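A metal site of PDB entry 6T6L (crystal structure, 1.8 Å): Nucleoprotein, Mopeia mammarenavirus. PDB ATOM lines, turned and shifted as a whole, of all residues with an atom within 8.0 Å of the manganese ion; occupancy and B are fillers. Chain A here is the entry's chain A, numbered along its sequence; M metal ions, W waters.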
ATOM      1  N   ILE A  25      -2.332  -1.119 -14.487  1.00  0.00           N
ATOM      2  CA  ILE A  25      -3.537  -0.303 -14.537  1.00  0.00           C
ATOM      3  C   ILE A  25      -3.775   0.143 -15.975  1.00  0.00           C
ATOM      4  O   ILE A  25      -2.831   0.454 -16.703  1.00  0.00           O
ATOM      5  CB  ILE A  25      -3.465   0.900 -13.578  1.00  0.00           C
ATOM      6  CG1 ILE A  25      -4.786   1.693 -13.590  1.00  0.00           C
ATOM      7  CG2 ILE A  25      -2.239   1.803 -13.880  1.00  0.00           C
ATOM      8  CD1 ILE A  25      -4.907   2.665 -12.391  1.00  0.00           C
ATOM      9  N   ASP A  26      -5.048   0.155 -16.367  1.00  0.00           N
ATOM     10  CA  ASP A  26      -5.425   0.604 -17.690  1.00  0.00           C
ATOM     11  C   ASP A  26      -6.799   1.235 -17.560  1.00  0.00           C
ATOM     12  O   ASP A  26      -7.621   0.762 -16.766  1.00  0.00           O
ATOM     13  CB  ASP A  26      -5.433  -0.576 -18.686  1.00  0.00           C
ATOM     14  CG  ASP A  26      -5.405  -0.127 -20.135  1.00  0.00           C
ATOM     15  OD1 ASP A  26      -4.328   0.222 -20.649  1.00  0.00           O
ATOM     16  OD2 ASP A  26      -6.476  -0.148 -20.764  1.00  0.00           O
ATOM     17  N   ILE A  27      -7.049   2.319 -18.304  1.00  0.00           N
ATOM     18  CA  ILE A  27      -8.364   2.945 -18.283  1.00  0.00           C
ATOM     19  C   ILE A  27      -8.835   3.157 -19.714  1.00  0.00           C
ATOM     20  O   ILE A  27      -8.028   3.301 -20.643  1.00  0.00           O
ATOM     21  CB  ILE A  27      -8.379   4.300 -17.514  1.00  0.00           C
ATOM     22  CG1 ILE A  27      -7.664   5.390 -18.332  1.00  0.00           C
ATOM     23  CG2 ILE A  27      -7.751   4.144 -16.126  1.00  0.00           C
ATOM     24  CD1 ILE A  27      -7.608   6.766 -17.608  1.00  0.00           C
ATOM     25  N   GLU A  28     -10.155   3.219 -19.898  1.00  0.00           N
ATOM     26  CA  GLU A  28     -10.722   3.694 -21.152  1.00  0.00           C
ATOM     27  C   GLU A  28     -11.493   4.967 -20.864  1.00  0.00           C
ATOM     28  O   GLU A  28     -12.072   5.112 -19.784  1.00  0.00           O
ATOM     29  CB  GLU A  28     -11.652   2.641 -21.804  1.00  0.00           C
ATOM     30  CG  GLU A  28     -10.971   1.277 -22.065  1.00  0.00           C
ATOM     31  CD  GLU A  28      -9.732   1.371 -22.942  1.00  0.00           C
ATOM     32  OE1 GLU A  28      -9.700   2.229 -23.866  1.00  0.00           O
ATOM     33  OE2 GLU A  28      -8.788   0.562 -22.727  1.00  0.00           O
ATOM     34  N   GLY A  29     -11.458   5.906 -21.812  1.00  0.00           N
ATOM     35  CA  GLY A  29     -11.983   7.257 -21.676  1.00  0.00           C
ATOM     36  C   GLY A  29     -10.909   8.253 -21.247  1.00  0.00           C
ATOM     37  O   GLY A  29      -9.843   7.897 -20.742  1.00  0.00           O
ATOM     38  N   GLU A  36     -14.011   3.126 -17.857  1.00  0.00           N
ATOM     39  CA  GLU A  36     -13.692   1.750 -17.507  1.00  0.00           C
ATOM     40  C   GLU A  36     -12.302   1.766 -16.912  1.00  0.00           C
ATOM     41  O   GLU A  36     -11.385   2.379 -17.475  1.00  0.00           O
ATOM     42  CB  GLU A  36     -13.766   0.804 -18.718  1.00  0.00           C
ATOM     43  CG  GLU A  36     -13.594  -0.660 -18.333  1.00  0.00           C
ATOM     44  CD  GLU A  36     -13.564  -1.582 -19.552  1.00  0.00           C
ATOM     45  OE1 GLU A  36     -13.099  -1.152 -20.622  1.00  0.00           O
ATOM     46  OE2 GLU A  36     -14.011  -2.741 -19.402  1.00  0.00           O
ATOM     47  N   SER A  67     -12.348   3.835 -29.734  1.00  0.00           N
ATOM     48  CA  SER A  67     -11.487   2.888 -29.008  1.00  0.00           C
ATOM     49  C   SER A  67     -12.287   1.795 -28.331  1.00  0.00           C
ATOM     50  O   SER A  67     -11.953   0.622 -28.486  1.00  0.00           O
ATOM     51  CB  SER A  67     -10.586   3.461 -27.939  1.00  0.00           C
ATOM     52  OG  SER A  67     -11.279   4.033 -26.877  1.00  0.00           O
ATOM     53  N   HIS A  68     -13.263   2.146 -27.469  1.00  0.00           N
ATOM     54  CA  HIS A  68     -13.769   1.088 -26.599  1.00  0.00           C
ATOM     55  C   HIS A  68     -15.074   0.453 -27.034  1.00  0.00           C
ATOM     56  O   HIS A  68     -15.382  -0.628 -26.536  1.00  0.00           O
ATOM     57  CB  HIS A  68     -13.918   1.569 -25.144  1.00  0.00           C
ATOM     58  CG  HIS A  68     -14.694   2.838 -24.987  1.00  0.00           C
ATOM     59  ND1 HIS A  68     -16.047   2.934 -25.258  1.00  0.00           N
ATOM     60  CD2 HIS A  68     -14.324   4.064 -24.534  1.00  0.00           C
ATOM     61  CE1 HIS A  68     -16.467   4.159 -24.990  1.00  0.00           C
ATOM     62  NE2 HIS A  68     -15.431   4.861 -24.558  1.00  0.00           N
ATOM     63  N   GLN A  99       0.664   0.744 -20.091  1.00  0.00           N
ATOM     64  CA  GLN A  99       1.091   1.033 -21.463  1.00  0.00           C
ATOM     65  C   GLN A  99       0.582   2.414 -21.864  1.00  0.00           C
ATOM     66  O   GLN A  99      -0.595   2.588 -22.173  1.00  0.00           O
ATOM     67  CB  GLN A  99       0.576  -0.087 -22.364  1.00  0.00           C
ATOM     68  CG  GLN A  99       0.651   0.191 -23.838  1.00  0.00           C
ATOM     69  CD  GLN A  99       2.065   0.041 -24.378  1.00  0.00           C
ATOM     70  OE1 GLN A  99       2.991  -0.315 -23.643  1.00  0.00           O
ATOM     71  NE2 GLN A  99       2.207   0.284 -25.663  1.00  0.00           N
ATOM     72  N   ILE A 104      -3.230   8.320 -17.273  1.00  0.00           N
ATOM     73  CA  ILE A 104      -3.422   7.792 -15.932  1.00  0.00           C
ATOM     74  C   ILE A 104      -2.702   8.659 -14.913  1.00  0.00           C
ATOM     75  O   ILE A 104      -3.193   8.843 -13.794  1.00  0.00           O
ATOM     76  CB  ILE A 104      -2.994   6.308 -15.905  1.00  0.00           C
ATOM     77  CG1 ILE A 104      -4.008   5.503 -16.724  1.00  0.00           C
ATOM     78  CG2 ILE A 104      -2.938   5.785 -14.472  1.00  0.00           C
ATOM     79  CD1 ILE A 104      -3.612   4.062 -16.978  1.00  0.00           C
ATOM     80  N   ARG A 129      -0.023  -5.473 -28.554  1.00  0.00           N
ATOM     81  CA  ARG A 129      -1.241  -6.223 -28.797  1.00  0.00           C
ATOM     82  C   ARG A 129      -0.994  -7.533 -29.538  1.00  0.00           C
ATOM     83  O   ARG A 129      -1.932  -8.093 -30.124  1.00  0.00           O
ATOM     84  CB  ARG A 129      -2.243  -5.343 -29.541  1.00  0.00           C
ATOM     85  CG  ARG A 129      -2.685  -4.157 -28.673  1.00  0.00           C
ATOM     86  CD  ARG A 129      -3.751  -3.280 -29.309  1.00  0.00           C
ATOM     87  NE  ARG A 129      -4.076  -2.200 -28.384  1.00  0.00           N
ATOM     88  CZ  ARG A 129      -4.968  -2.303 -27.403  1.00  0.00           C
ATOM     89  NH1 ARG A 129      -5.663  -3.428 -27.240  1.00  0.00           N
ATOM     90  NH2 ARG A 129      -5.155  -1.276 -26.590  1.00  0.00           N
ATOM     91  N   PRO A 164     -12.225  -3.813 -30.235  1.00  0.00           N
ATOM     92  CA  PRO A 164     -12.418  -2.781 -29.211  1.00  0.00           C
ATOM     93  C   PRO A 164     -11.419  -2.930 -28.078  1.00  0.00           C
ATOM     94  O   PRO A 164     -10.923  -4.028 -27.791  1.00  0.00           O
ATOM     95  CB  PRO A 164     -13.849  -3.013 -28.739  1.00  0.00           C
ATOM     96  CG  PRO A 164     -14.532  -3.633 -29.940  1.00  0.00           C
ATOM     97  CD  PRO A 164     -13.475  -4.515 -30.569  1.00  0.00           C
ATOM     98  N   HIS A 165     -11.099  -1.802 -27.438  1.00  0.00           N
ATOM     99  CA  HIS A 165     -10.192  -1.791 -26.298  1.00  0.00           C
ATOM    100  C   HIS A 165     -10.983  -1.897 -24.997  1.00  0.00           C
ATOM    101  O   HIS A 165     -11.836  -1.054 -24.694  1.00  0.00           O
ATOM    102  CB  HIS A 165      -9.349  -0.515 -26.336  1.00  0.00           C
ATOM    103  CG  HIS A 165      -8.410  -0.440 -27.504  1.00  0.00           C
ATOM    104  ND1 HIS A 165      -7.618   0.656 -27.752  1.00  0.00           N
ATOM    105  CD2 HIS A 165      -8.132  -1.342 -28.483  1.00  0.00           C
ATOM    106  CE1 HIS A 165      -6.885   0.432 -28.834  1.00  0.00           C
ATOM    107  NE2 HIS A 165      -7.180  -0.771 -29.302  1.00  0.00           N
ATOM    108  N   CYS A 166     -10.643  -2.896 -24.202  1.00  0.00           N
ATOM    109  CA  CYS A 166     -11.195  -3.104 -22.871  1.00  0.00           C
ATOM    110  C   CYS A 166     -10.069  -2.937 -21.851  1.00  0.00           C
ATOM    111  O   CYS A 166      -8.970  -3.482 -22.045  1.00  0.00           O
ATOM    112  CB  CYS A 166     -11.782  -4.534 -22.801  1.00  0.00           C
ATOM    113  SG  CYS A 166     -12.073  -5.202 -21.102  1.00  0.00           S
ATOM    114  N   ALA A 167     -10.328  -2.169 -20.802  1.00  0.00           N
ATOM    115  CA  ALA A 167      -9.251  -1.882 -19.857  1.00  0.00           C
ATOM    116  C   ALA A 167      -8.734  -3.171 -19.223  1.00  0.00           C
ATOM    117  O   ALA A 167      -7.532  -3.306 -18.999  1.00  0.00           O
ATOM    118  CB  ALA A 167      -9.717  -0.894 -18.788  1.00  0.00           C
ATOM    119  N   LEU A 168      -9.637  -4.130 -18.973  1.00  0.00           N
ATOM    120  CA  LEU A 168      -9.218  -5.371 -18.336  1.00  0.00           C
ATOM    121  C   LEU A 168      -8.430  -6.244 -19.308  1.00  0.00           C
ATOM    122  O   LEU A 168      -7.338  -6.706 -18.981  1.00  0.00           O
ATOM    123  CB  LEU A 168     -10.423  -6.139 -17.806  1.00  0.00           C
ATOM    124  CG  LEU A 168     -10.123  -7.543 -17.282  1.00  0.00           C
ATOM    125  CD1 LEU A 168      -9.118  -7.508 -16.127  1.00  0.00           C
ATOM    126  CD2 LEU A 168     -11.435  -8.236 -16.881  1.00  0.00           C
ATOM    127  N   LEU A 169      -8.974  -6.486 -20.491  1.00  0.00           N
ATOM    128  CA  LEU A 169      -8.269  -7.389 -21.398  1.00  0.00           C
ATOM    129  C   LEU A 169      -6.987  -6.750 -21.907  1.00  0.00           C
ATOM    130  O   LEU A 169      -6.020  -7.463 -22.207  1.00  0.00           O
ATOM    131  CB  LEU A 169      -9.200  -7.806 -22.540  1.00  0.00           C
ATOM    132  CG  LEU A 169      -9.970  -9.132 -22.266  1.00  0.00           C
ATOM    133  CD1 LEU A 169     -10.694  -9.129 -20.938  1.00  0.00           C
ATOM    134  CD2 LEU A 169     -10.955  -9.443 -23.405  1.00  0.00           C
ATOM    135  N   ASP A 170      -6.928  -5.416 -21.963  1.00  0.00           N
ATOM    136  CA  ASP A 170      -5.669  -4.744 -22.269  1.00  0.00           C
ATOM    137  C   ASP A 170      -4.600  -5.079 -21.229  1.00  0.00           C
ATOM    138  O   ASP A 170      -3.471  -5.442 -21.576  1.00  0.00           O
ATOM    139  CB  ASP A 170      -5.864  -3.227 -22.380  1.00  0.00           C
ATOM    140  CG  ASP A 170      -6.467  -2.796 -23.710  1.00  0.00           C
ATOM    141  OD1 ASP A 170      -6.679  -3.669 -24.572  1.00  0.00           O
ATOM    142  OD2 ASP A 170      -6.728  -1.591 -23.910  1.00  0.00           O
ATOM    143  N   CYS A 171      -4.939  -4.980 -19.932  1.00  0.00           N
ATOM    144  CA  CYS A 171      -3.994  -5.423 -18.898  1.00  0.00           C
ATOM    145  C   CYS A 171      -3.541  -6.859 -19.149  1.00  0.00           C
ATOM    146  O   CYS A 171      -2.349  -7.169 -19.068  1.00  0.00           O
ATOM    147  CB  CYS A 171      -4.601  -5.360 -17.503  1.00  0.00           C
ATOM    148  SG  CYS A 171      -4.853  -3.693 -16.832  1.00  0.00           S
ATOM    149  N   MET A 173      -3.514  -8.741 -21.907  1.00  0.00           N
ATOM    150  CA  MET A 173      -2.676  -8.946 -23.085  1.00  0.00           C
ATOM    151  C   MET A 173      -1.348  -8.200 -22.965  1.00  0.00           C
ATOM    152  O   MET A 173      -0.342  -8.647 -23.529  1.00  0.00           O
ATOM    153  CB  MET A 173      -3.441  -8.523 -24.340  1.00  0.00           C
ATOM    154  CG  MET A 173      -3.404  -7.024 -24.634  1.00  0.00           C
ATOM    155  SD  MET A 173      -4.342  -6.637 -26.146  1.00  0.00           S
ATOM    156  CE  MET A 173      -6.012  -6.923 -25.538  1.00  0.00           C
ATOM    157  N   PHE A 174      -1.294  -7.084 -22.223  1.00  0.00           N
ATOM    158  CA  PHE A 174       0.002  -6.433 -22.031  1.00  0.00           C
ATOM    159  C   PHE A 174       0.928  -7.311 -21.216  1.00  0.00           C
ATOM    160  O   PHE A 174       2.122  -7.447 -21.537  1.00  0.00           O
ATOM    161  CB  PHE A 174      -0.167  -5.057 -21.384  1.00  0.00           C
ATOM    162  CG  PHE A 174      -0.946  -4.067 -22.229  1.00  0.00           C
ATOM    163  CD1 PHE A 174      -1.053  -4.227 -23.605  1.00  0.00           C
ATOM    164  CD2 PHE A 174      -1.598  -2.984 -21.649  1.00  0.00           C
ATOM    165  CE1 PHE A 174      -1.771  -3.328 -24.376  1.00  0.00           C
ATOM    166  CE2 PHE A 174      -2.345  -2.090 -22.415  1.00  0.00           C
ATOM    167  CZ  PHE A 174      -2.435  -2.257 -23.763  1.00  0.00           C
HETATM  168 MN    MN M   1      -6.814   0.292 -22.968  1.00  0.00          MN
HETATM  169  O   HOH W   1      -4.511   0.552 -23.204  1.00  0.00           O
HETATM  170  O   HOH W   2      -6.477   2.349 -22.284  1.00  0.00           O
HETATM  171  O   HOH W   3      -7.014   1.874 -24.800  1.00  0.00           O
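The backbone NH of Glu 28 is in hydrogen-bond range of the backbone carbonyl oxygen of Glu 36 (2.8 Å).
The side-chain carboxylate (OD1) of Asp 170 lies within salt-bridge range of the guanidinium group (NH1) of Arg 129 (2.9 Å).
Merely in contact with the manganese ion: Ile 27 (3.99 Å).
Four residues have an atom within 4 Å of the manganese ion: Asp 26, Ile 27, Glu 28 and Asp 170.
The manganese ion is bound by OE2 of Glu 28 (2.0 Å), OD2 of Asp 170 (2.1 Å), water W2 (2.2 Å), OD2 of Asp 26 (2.3 Å), water W1 (2.3 Å) and water W3 (2.4 Å).
Water W3 lies within hydrogen-bond range of the side-chain carboxylate (OE1) of Glu 28 and a ring nitrogen (ND1) of His 165.
Water W2 bridges O of Ile 27 (2.5 Å) and OD1 of Asp 26 (3.4 Å).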
